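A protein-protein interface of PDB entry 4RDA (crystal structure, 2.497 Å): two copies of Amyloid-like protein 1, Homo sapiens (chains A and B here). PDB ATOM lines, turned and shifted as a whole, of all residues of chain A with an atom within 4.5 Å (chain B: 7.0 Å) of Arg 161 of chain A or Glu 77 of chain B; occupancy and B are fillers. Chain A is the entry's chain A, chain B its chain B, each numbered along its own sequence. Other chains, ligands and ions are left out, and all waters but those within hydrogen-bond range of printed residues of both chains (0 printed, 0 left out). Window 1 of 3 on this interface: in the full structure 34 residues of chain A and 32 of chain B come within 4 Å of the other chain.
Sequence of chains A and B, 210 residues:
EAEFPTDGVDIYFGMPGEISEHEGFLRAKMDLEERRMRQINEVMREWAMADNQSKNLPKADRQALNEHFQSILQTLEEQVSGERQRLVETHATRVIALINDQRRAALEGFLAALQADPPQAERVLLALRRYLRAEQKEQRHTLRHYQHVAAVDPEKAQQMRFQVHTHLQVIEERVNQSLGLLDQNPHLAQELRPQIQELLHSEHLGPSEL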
ATOM      1  N   TYR A 146      23.625  20.037 -19.887  1.00  0.00           N
ATOM      2  CA  TYR A 146      24.271  19.665 -18.632  1.00  0.00           C
ATOM      3  C   TYR A 146      25.755  20.016 -18.702  1.00  0.00           C
ATOM      4  O   TYR A 146      26.324  20.553 -17.759  1.00  0.00           O
ATOM      5  CB  TYR A 146      24.085  18.175 -18.339  1.00  0.00           C
ATOM      6  CG  TYR A 146      24.879  17.678 -17.144  1.00  0.00           C
ATOM      7  CD1 TYR A 146      24.813  18.336 -15.912  1.00  0.00           C
ATOM      8  CD2 TYR A 146      25.688  16.556 -17.243  1.00  0.00           C
ATOM      9  CE1 TYR A 146      25.536  17.890 -14.822  1.00  0.00           C
ATOM     10  CE2 TYR A 146      26.414  16.100 -16.155  1.00  0.00           C
ATOM     11  CZ  TYR A 146      26.335  16.771 -14.950  1.00  0.00           C
ATOM     12  OH  TYR A 146      27.057  16.321 -13.873  1.00  0.00           O
ATOM     13  N   ALA A 150      27.748  22.795 -16.450  1.00  0.00           N
ATOM     14  CA  ALA A 150      28.943  22.390 -15.725  1.00  0.00           C
ATOM     15  C   ALA A 150      30.120  23.321 -16.065  1.00  0.00           C
ATOM     16  O   ALA A 150      30.951  23.642 -15.212  1.00  0.00           O
ATOM     17  CB  ALA A 150      29.290  20.950 -16.049  1.00  0.00           C
ATOM     18  N   ALA A 157      25.283  22.970 -11.737  1.00  0.00           N
ATOM     19  CA  ALA A 157      25.452  21.649 -12.333  1.00  0.00           C
ATOM     20  C   ALA A 157      25.122  20.534 -11.350  1.00  0.00           C
ATOM     21  O   ALA A 157      24.385  19.605 -11.682  1.00  0.00           O
ATOM     22  CB  ALA A 157      26.863  21.489 -12.841  1.00  0.00           C
ATOM     23  N   GLN A 158      25.681  20.638 -10.149  1.00  0.00           N
ATOM     24  CA  GLN A 158      25.431  19.688  -9.073  1.00  0.00           C
ATOM     25  C   GLN A 158      23.940  19.583  -8.765  1.00  0.00           C
ATOM     26  O   GLN A 158      23.461  18.522  -8.397  1.00  0.00           O
ATOM     27  CB  GLN A 158      26.219  20.092  -7.820  1.00  0.00           C
ATOM     28  CG  GLN A 158      25.937  19.268  -6.563  1.00  0.00           C
ATOM     29  CD  GLN A 158      24.797  19.835  -5.727  1.00  0.00           C
ATOM     30  N   GLN A 159      23.200  20.673  -8.930  1.00  0.00           N
ATOM     31  CA  GLN A 159      21.755  20.647  -8.706  1.00  0.00           C
ATOM     32  C   GLN A 159      21.003  19.809  -9.745  1.00  0.00           C
ATOM     33  O   GLN A 159      19.876  19.384  -9.497  1.00  0.00           O
ATOM     34  CB  GLN A 159      21.181  22.065  -8.720  1.00  0.00           C
ATOM     35  CG  GLN A 159      21.587  22.955  -7.557  1.00  0.00           C
ATOM     36  N   MET A 160      21.625  19.609 -10.909  1.00  0.00           N
ATOM     37  CA  MET A 160      20.995  18.976 -12.063  1.00  0.00           C
ATOM     38  C   MET A 160      21.201  17.461 -12.142  1.00  0.00           C
ATOM     39  O   MET A 160      20.307  16.752 -12.596  1.00  0.00           O
ATOM     40  CB  MET A 160      21.530  19.565 -13.365  1.00  0.00           C
ATOM     41  CG  MET A 160      21.285  21.005 -13.620  1.00  0.00           C
ATOM     42  SD  MET A 160      22.277  21.464 -15.057  1.00  0.00           S
ATOM     43  CE  MET A 160      21.346  20.758 -16.407  1.00  0.00           C
ATOM     44  N   ARG A 161      22.387  16.999 -11.739  1.00  0.00           N
ATOM     45  CA  ARG A 161      22.840  15.624 -11.954  1.00  0.00           C
ATOM     46  C   ARG A 161      21.746  14.571 -11.971  1.00  0.00           C
ATOM     47  O   ARG A 161      21.491  13.936 -12.994  1.00  0.00           O
ATOM     48  CB  ARG A 161      23.835  15.223 -10.882  1.00  0.00           C
ATOM     49  CG  ARG A 161      25.140  15.910 -10.973  1.00  0.00           C
ATOM     50  CD  ARG A 161      25.919  15.576  -9.740  1.00  0.00           C
ATOM     51  NE  ARG A 161      26.967  16.548  -9.485  1.00  0.00           N
ATOM     52  CZ  ARG A 161      27.622  16.616  -8.340  1.00  0.00           C
ATOM     53  NH1 ARG A 161      27.310  15.775  -7.368  1.00  0.00           N
ATOM     54  NH2 ARG A 161      28.574  17.520  -8.169  1.00  0.00           N
ATOM     55  N   PHE A 162      21.106  14.396 -10.825  1.00  0.00           N
ATOM     56  CA  PHE A 162      20.072  13.395 -10.686  1.00  0.00           C
ATOM     57  C   PHE A 162      18.969  13.555 -11.735  1.00  0.00           C
ATOM     58  O   PHE A 162      18.545  12.579 -12.351  1.00  0.00           O
ATOM     59  CB  PHE A 162      19.477  13.442  -9.282  1.00  0.00           C
ATOM     60  CG  PHE A 162      18.679  12.239  -8.950  1.00  0.00           C
ATOM     61  CD1 PHE A 162      19.305  11.097  -8.470  1.00  0.00           C
ATOM     62  CD2 PHE A 162      17.309  12.217  -9.170  1.00  0.00           C
ATOM     63  CE1 PHE A 162      18.573   9.956  -8.191  1.00  0.00           C
ATOM     64  CE2 PHE A 162      16.570  11.081  -8.892  1.00  0.00           C
ATOM     65  CZ  PHE A 162      17.201   9.949  -8.400  1.00  0.00           C
ATOM     66  N   GLN A 163      18.517  14.782 -11.947  1.00  0.00           N
ATOM     67  CA  GLN A 163      17.459  15.055 -12.909  1.00  0.00           C
ATOM     68  C   GLN A 163      17.872  14.678 -14.343  1.00  0.00           C
ATOM     69  O   GLN A 163      17.076  14.110 -15.097  1.00  0.00           O
ATOM     70  CB  GLN A 163      17.070  16.518 -12.812  1.00  0.00           C
ATOM     71  CG  GLN A 163      16.454  17.108 -14.051  1.00  0.00           C
ATOM     72  N   VAL A 164      19.121  14.992 -14.694  1.00  0.00           N
ATOM     73  CA  VAL A 164      19.724  14.627 -15.976  1.00  0.00           C
ATOM     74  C   VAL A 164      19.766  13.112 -16.112  1.00  0.00           C
ATOM     75  O   VAL A 164      19.417  12.529 -17.152  1.00  0.00           O
ATOM     76  CB  VAL A 164      21.173  15.187 -16.104  1.00  0.00           C
ATOM     77  CG1 VAL A 164      21.878  14.618 -17.341  1.00  0.00           C
ATOM     78  CG2 VAL A 164      21.187  16.724 -16.101  1.00  0.00           C
ATOM     79  N   HIS A 165      20.217  12.487 -15.037  1.00  0.00           N
ATOM     80  CA  HIS A 165      20.369  11.046 -14.949  1.00  0.00           C
ATOM     81  C   HIS A 165      19.021  10.346 -15.168  1.00  0.00           C
ATOM     82  O   HIS A 165      18.924   9.359 -15.904  1.00  0.00           O
ATOM     83  CB  HIS A 165      20.984  10.716 -13.596  1.00  0.00           C
ATOM     84  CG  HIS A 165      20.787   9.309 -13.142  1.00  0.00           C
ATOM     85  ND1 HIS A 165      21.492   8.249 -13.673  1.00  0.00           N
ATOM     86  CD2 HIS A 165      20.017   8.795 -12.158  1.00  0.00           C
ATOM     87  CE1 HIS A 165      21.135   7.137 -13.055  1.00  0.00           C
ATOM     88  NE2 HIS A 165      20.243   7.443 -12.129  1.00  0.00           N
ATOM     89  N   ARG B  36      33.425  15.807 -23.910  1.00  0.00           N
ATOM     90  CA  ARG B  36      32.869  15.758 -22.549  1.00  0.00           C
ATOM     91  C   ARG B  36      31.442  15.193 -22.471  1.00  0.00           C
ATOM     92  O   ARG B  36      31.042  14.656 -21.444  1.00  0.00           O
ATOM     93  CB  ARG B  36      32.878  17.156 -21.920  1.00  0.00           C
ATOM     94  CG  ARG B  36      34.253  17.717 -21.661  1.00  0.00           C
ATOM     95  CD  ARG B  36      35.025  16.861 -20.681  1.00  0.00           C
ATOM     96  NE  ARG B  36      36.286  17.491 -20.312  1.00  0.00           N
ATOM     97  CZ  ARG B  36      37.082  17.050 -19.344  1.00  0.00           C
ATOM     98  NH1 ARG B  36      36.745  15.970 -18.646  1.00  0.00           N
ATOM     99  NH2 ARG B  36      38.211  17.693 -19.068  1.00  0.00           N
ATOM    100  N   ILE B  40      30.304  12.055 -19.994  1.00  0.00           N
ATOM    101  CA  ILE B  40      29.135  12.166 -19.154  1.00  0.00           C
ATOM    102  C   ILE B  40      28.122  11.085 -19.508  1.00  0.00           C
ATOM    103  O   ILE B  40      27.515  10.500 -18.625  1.00  0.00           O
ATOM    104  CB  ILE B  40      28.498  13.553 -19.267  1.00  0.00           C
ATOM    105  CG1 ILE B  40      29.509  14.616 -18.852  1.00  0.00           C
ATOM    106  CG2 ILE B  40      27.244  13.640 -18.401  1.00  0.00           C
ATOM    107  CD1 ILE B  40      29.014  16.032 -19.044  1.00  0.00           C
ATOM    108  N   MET B  44      26.733   8.296 -16.895  1.00  0.00           N
ATOM    109  CA  MET B  44      25.294   8.276 -16.642  1.00  0.00           C
ATOM    110  C   MET B  44      24.718   6.892 -16.875  1.00  0.00           C
ATOM    111  O   MET B  44      23.770   6.486 -16.208  1.00  0.00           O
ATOM    112  CB  MET B  44      24.568   9.302 -17.525  1.00  0.00           C
ATOM    113  CG  MET B  44      24.789  10.756 -17.113  1.00  0.00           C
ATOM    114  SD  MET B  44      23.937  11.146 -15.584  1.00  0.00           S
ATOM    115  CE  MET B  44      24.458  12.845 -15.322  1.00  0.00           C
ATOM    116  N   TRP B  47      25.811   4.534 -14.134  1.00  0.00           N
ATOM    117  CA  TRP B  47      24.986   4.869 -12.982  1.00  0.00           C
ATOM    118  C   TRP B  47      23.643   4.180 -13.089  1.00  0.00           C
ATOM    119  O   TRP B  47      23.170   3.607 -12.119  1.00  0.00           O
ATOM    120  CB  TRP B  47      24.803   6.388 -12.868  1.00  0.00           C
ATOM    121  CG  TRP B  47      24.126   6.853 -11.599  1.00  0.00           C
ATOM    122  CD1 TRP B  47      23.667   6.073 -10.576  1.00  0.00           C
ATOM    123  CD2 TRP B  47      23.847   8.210 -11.219  1.00  0.00           C
ATOM    124  NE1 TRP B  47      23.120   6.856  -9.589  1.00  0.00           N
ATOM    125  CE2 TRP B  47      23.220   8.174  -9.957  1.00  0.00           C
ATOM    126  CE3 TRP B  47      24.069   9.456 -11.823  1.00  0.00           C
ATOM    127  CZ2 TRP B  47      22.806   9.326  -9.293  1.00  0.00           C
ATOM    128  CZ3 TRP B  47      23.658  10.597 -11.164  1.00  0.00           C
ATOM    129  CH2 TRP B  47      23.031  10.525  -9.914  1.00  0.00           C
ATOM    130  N   GLU B  67      25.557   8.330  -4.067  1.00  0.00           N
ATOM    131  CA  GLU B  67      26.601   9.272  -3.703  1.00  0.00           C
ATOM    132  C   GLU B  67      27.887   8.959  -4.460  1.00  0.00           C
ATOM    133  O   GLU B  67      28.678   9.860  -4.740  1.00  0.00           O
ATOM    134  CB  GLU B  67      26.841   9.265  -2.189  1.00  0.00           C
ATOM    135  N   PHE B  69      28.361   7.916  -7.645  1.00  0.00           N
ATOM    136  CA  PHE B  69      28.364   8.493  -8.983  1.00  0.00           C
ATOM    137  C   PHE B  69      28.267  10.014  -8.927  1.00  0.00           C
ATOM    138  O   PHE B  69      28.877  10.707  -9.744  1.00  0.00           O
ATOM    139  CB  PHE B  69      27.231   7.896  -9.820  1.00  0.00           C
ATOM    140  CG  PHE B  69      27.487   6.478 -10.219  1.00  0.00           C
ATOM    141  CD1 PHE B  69      28.298   6.192 -11.304  1.00  0.00           C
ATOM    142  CD2 PHE B  69      26.962   5.431  -9.485  1.00  0.00           C
ATOM    143  CE1 PHE B  69      28.568   4.894 -11.662  1.00  0.00           C
ATOM    144  CE2 PHE B  69      27.224   4.125  -9.840  1.00  0.00           C
ATOM    145  CZ  PHE B  69      28.029   3.857 -10.933  1.00  0.00           C
ATOM    146  N   GLN B  70      27.507  10.522  -7.961  1.00  0.00           N
ATOM    147  CA  GLN B  70      27.467  11.954  -7.679  1.00  0.00           C
ATOM    148  C   GLN B  70      28.876  12.497  -7.471  1.00  0.00           C
ATOM    149  O   GLN B  70      29.250  13.519  -8.040  1.00  0.00           O
ATOM    150  CB  GLN B  70      26.601  12.233  -6.453  1.00  0.00           C
ATOM    151  CG  GLN B  70      25.122  11.999  -6.696  1.00  0.00           C
ATOM    152  CD  GLN B  70      24.326  13.288  -6.719  1.00  0.00           C
ATOM    153  OE1 GLN B  70      24.893  14.387  -6.664  1.00  0.00           O
ATOM    154  NE2 GLN B  70      23.001  13.164  -6.790  1.00  0.00           N
ATOM    155  N   SER B  71      29.658  11.786  -6.669  1.00  0.00           N
ATOM    156  CA  SER B  71      31.067  12.103  -6.475  1.00  0.00           C
ATOM    157  C   SER B  71      31.868  12.066  -7.776  1.00  0.00           C
ATOM    158  O   SER B  71      32.689  12.945  -8.034  1.00  0.00           O
ATOM    159  CB  SER B  71      31.678  11.128  -5.471  1.00  0.00           C
ATOM    160  OG  SER B  71      33.068  10.972  -5.707  1.00  0.00           O
ATOM    161  N   ILE B  72      31.632  11.029  -8.581  1.00  0.00           N
ATOM    162  CA  ILE B  72      32.299  10.874  -9.872  1.00  0.00           C
ATOM    163  C   ILE B  72      32.010  12.062 -10.778  1.00  0.00           C
ATOM    164  O   ILE B  72      32.922  12.627 -11.382  1.00  0.00           O
ATOM    165  CB  ILE B  72      31.861   9.575 -10.611  1.00  0.00           C
ATOM    166  CG1 ILE B  72      32.342   8.326  -9.865  1.00  0.00           C
ATOM    167  CG2 ILE B  72      32.381   9.573 -12.052  1.00  0.00           C
ATOM    168  N   LEU B  73      30.736  12.432 -10.862  1.00  0.00           N
ATOM    169  CA  LEU B  73      30.302  13.523 -11.728  1.00  0.00           C
ATOM    170  C   LEU B  73      30.850  14.871 -11.234  1.00  0.00           C
ATOM    171  O   LEU B  73      31.233  15.737 -12.031  1.00  0.00           O
ATOM    172  CB  LEU B  73      28.766  13.551 -11.825  1.00  0.00           C
ATOM    173  CG  LEU B  73      28.109  12.375 -12.569  1.00  0.00           C
ATOM    174  CD1 LEU B  73      26.598  12.365 -12.392  1.00  0.00           C
ATOM    175  CD2 LEU B  73      28.430  12.397 -14.049  1.00  0.00           C
ATOM    176  N   GLN B  74      30.916  15.041  -9.922  1.00  0.00           N
ATOM    177  CA  GLN B  74      31.462  16.275  -9.375  1.00  0.00           C
ATOM    178  C   GLN B  74      32.902  16.497  -9.828  1.00  0.00           C
ATOM    179  O   GLN B  74      33.285  17.609 -10.182  1.00  0.00           O
ATOM    180  CB  GLN B  74      31.400  16.270  -7.861  1.00  0.00           C
ATOM    181  CG  GLN B  74      31.883  17.573  -7.266  1.00  0.00           C
ATOM    182  CD  GLN B  74      31.910  17.531  -5.768  1.00  0.00           C
ATOM    183  OE1 GLN B  74      30.868  17.617  -5.120  1.00  0.00           O
ATOM    184  NE2 GLN B  74      33.099  17.374  -5.200  1.00  0.00           N
ATOM    185  N   THR B  75      33.696  15.435  -9.826  1.00  0.00           N
ATOM    186  CA  THR B  75      35.050  15.520 -10.363  1.00  0.00           C
ATOM    187  C   THR B  75      34.997  15.908 -11.829  1.00  0.00           C
ATOM    188  O   THR B  75      35.821  16.684 -12.306  1.00  0.00           O
ATOM    189  CB  THR B  75      35.802  14.192 -10.229  1.00  0.00           C
ATOM    190  OG1 THR B  75      35.684  13.718  -8.886  1.00  0.00           O
ATOM    191  CG2 THR B  75      37.264  14.365 -10.576  1.00  0.00           C
ATOM    192  N   LEU B  76      34.008  15.369 -12.536  1.00  0.00           N
ATOM    193  CA  LEU B  76      33.875  15.615 -13.963  1.00  0.00           C
ATOM    194  C   LEU B  76      33.477  17.068 -14.235  1.00  0.00           C
ATOM    195  O   LEU B  76      34.059  17.725 -15.098  1.00  0.00           O
ATOM    196  CB  LEU B  76      32.857  14.656 -14.568  1.00  0.00           C
ATOM    197  CG  LEU B  76      33.197  14.004 -15.906  1.00  0.00           C
ATOM    198  CD1 LEU B  76      31.948  13.398 -16.492  1.00  0.00           C
ATOM    199  CD2 LEU B  76      33.786  15.004 -16.871  1.00  0.00           C
ATOM    200  N   GLU B  77      32.488  17.560 -13.497  1.00  0.00           N
ATOM    201  CA  GLU B  77      32.097  18.962 -13.589  1.00  0.00           C
ATOM    202  C   GLU B  77      33.290  19.873 -13.341  1.00  0.00           C
ATOM    203  O   GLU B  77      33.511  20.829 -14.083  1.00  0.00           O
ATOM    204  CB  GLU B  77      30.973  19.266 -12.604  1.00  0.00           C
ATOM    205  CG  GLU B  77      29.688  18.532 -12.948  1.00  0.00           C
ATOM    206  CD  GLU B  77      28.809  18.272 -11.747  1.00  0.00           C
ATOM    207  OE1 GLU B  77      29.259  18.473 -10.601  1.00  0.00           O
ATOM    208  OE2 GLU B  77      27.658  17.849 -11.950  1.00  0.00           O
ATOM    209  N   GLU B  78      34.075  19.549 -12.323  1.00  0.00           N
ATOM    210  CA  GLU B  78      35.246  20.347 -11.999  1.00  0.00           C
ATOM    211  C   GLU B  78      36.217  20.401 -13.160  1.00  0.00           C
ATOM    212  O   GLU B  78      36.657  21.484 -13.553  1.00  0.00           O
ATOM    213  CB  GLU B  78      35.935  19.803 -10.757  1.00  0.00           C
ATOM    214  CG  GLU B  78      35.225  20.181  -9.476  1.00  0.00           C
ATOM    215  CD  GLU B  78      35.757  19.433  -8.274  1.00  0.00           C
ATOM    216  OE1 GLU B  78      36.804  18.751  -8.403  1.00  0.00           O
ATOM    217  OE2 GLU B  78      35.116  19.526  -7.202  1.00  0.00           O
ATOM    218  N   GLN B  79      36.532  19.240 -13.724  1.00  0.00           N
ATOM    219  CA  GLN B  79      37.419  19.179 -14.879  1.00  0.00           C
ATOM    220  C   GLN B  79      36.875  19.976 -16.064  1.00  0.00           C
ATOM    221  O   GLN B  79      37.621  20.722 -16.713  1.00  0.00           O
ATOM    222  CB  GLN B  79      37.664  17.729 -15.290  1.00  0.00           C
ATOM    223  CG  GLN B  79      38.530  16.962 -14.312  1.00  0.00           C
ATOM    224  CD  GLN B  79      38.634  15.471 -14.647  1.00  0.00           C
ATOM    225  OE1 GLN B  79      38.283  15.028 -15.750  1.00  0.00           O
ATOM    226  NE2 GLN B  79      39.125  14.692 -13.687  1.00  0.00           N
ATOM    227  N   VAL B  80      35.581  19.830 -16.343  1.00  0.00           N
ATOM    228  CA  VAL B  80      34.953  20.585 -17.423  1.00  0.00           C
ATOM    229  C   VAL B  80      35.048  22.098 -17.171  1.00  0.00           C
ATOM    230  O   VAL B  80      35.433  22.866 -18.054  1.00  0.00           O
ATOM    231  CB  VAL B  80      33.477  20.191 -17.602  1.00  0.00           C
ATOM    232  CG1 VAL B  80      32.793  21.110 -18.602  1.00  0.00           C
ATOM    233  CG2 VAL B  80      33.374  18.758 -18.050  1.00  0.00           C
ATOM    234  N   SER B  81      34.713  22.520 -15.960  1.00  0.00           N
ATOM    235  CA  SER B  81      34.761  23.938 -15.598  1.00  0.00           C
ATOM    236  C   SER B  81      36.167  24.564 -15.714  1.00  0.00           C
ATOM    237  O   SER B  81      36.337  25.637 -16.307  1.00  0.00           O
ATOM    238  CB  SER B  81      34.241  24.119 -14.182  1.00  0.00           C
ATOM    239  OG  SER B  81      34.413  25.458 -13.809  1.00  0.00           O
ATOM    240  N   GLY B  82      37.165  23.890 -15.145  1.00  0.00           N
ATOM    241  CA  GLY B  82      38.543  24.333 -15.221  1.00  0.00           C
ATOM    242  C   GLY B  82      39.051  24.427 -16.640  1.00  0.00           C
ATOM    243  O   GLY B  82      39.740  25.371 -17.002  1.00  0.00           O
ATOM    244  N   GLU B  83      38.692  23.447 -17.456  1.00  0.00           N
ATOM    245  CA  GLU B  83      39.112  23.412 -18.845  1.00  0.00           C
ATOM    246  C   GLU B  83      38.522  24.562 -19.667  1.00  0.00           C
ATOM    247  O   GLU B  83      39.213  25.187 -20.466  1.00  0.00           O
ATOM    248  CB  GLU B  83      38.725  22.062 -19.420  1.00  0.00           C
ATOM    249  CG  GLU B  83      38.841  21.894 -20.896  1.00  0.00           C
ATOM    250  CD  GLU B  83      38.529  20.452 -21.281  1.00  0.00           C
ATOM    251  OE1 GLU B  83      39.462  19.618 -21.247  1.00  0.00           O
ATOM    252  OE2 GLU B  83      37.355  20.146 -21.575  1.00  0.00           O
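OH of Tyr 146 of chain A is in hydrogen-bond range of OE2 of Glu 77 of chain B (2.5 Å).
OE1 of Gln 70 of chain B lies within hydrogen-bond range of NH1 of Arg 161 of chain A (2.9 Å).
OE1 of Glu 77 of chain B is in salt-bridge range of NH2 of Arg 161 of chain A (2.7 Å).
No position is printed for both chains.
Of the 15 pairs that touch across the chains among the printed residues, none has its exchanged pair printed and touching as well.
Tyr 146 of chain A touches Met 44 of chain B.
Tyr 146 of chain A touches Leu 73 of chain B.
CG of Glu 77 of chain B touches CB of Ala 150 of chain A (3.95 Å).
O of Ala 150 of chain A touches CB of Ser 81 of chain B, 3.5 Å away.
Ala 157 of chain A touches Glu 77 of chain B (O to OE2, 3.7 Å).
Gln 158 of chain A touches Glu 77 of chain B (N to OE2, 3.9 Å).
Met 44 of chain B touches Arg 161 of chain A.
Gln 74 of chain B touches Arg 161 of chain A (CB to NH2, 3.1 Å).
CG1 of Val 164 of chain A touches CE of Met 44 of chain B (3.7 Å).
Trp 47 of chain B touches His 165 of chain A (CG to CE1, 3.3 Å).
Of the 20 printed residues of chain B, 8 touch a printed residue of chain A.
Hydrophobic or aromatic side chains of chain B within 4 Å of the printed part of chain A: Ile 40, Met 44, Trp 47 and Leu 73.
Of chain B, only Met 44 (3.9 Å), Gln 70 (2.9 Å), Gln 74 (3.1 Å) and Glu 77 (2.7 Å) come within 4 Å of Arg 161 of chain A.
Glu 77 of chain B touches five residues of chain A.
Of the printed residues of chain B, Ala 150 of chain A touches Glu 77 (3.95 Å) and Ser 81 (3.5 Å).
Of the printed residues of chain A, Gln 74 of chain B touches Arg 161.
Of the printed residues of chain A, Leu 73 of chain B touches Tyr 146 (3.8 Å).
Of the printed residues of chain A, Trp 47 of chain B touches His 165 (3.3 Å).
Printed residues of chain A within 4 Å of Met 44 of chain B: Tyr 146, Arg 161, Val 164 and His 165.
Val 80 of chain B touches none of the printed residues of chain A.
Glu 83 of chain B touches none of the printed residues of chain A.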
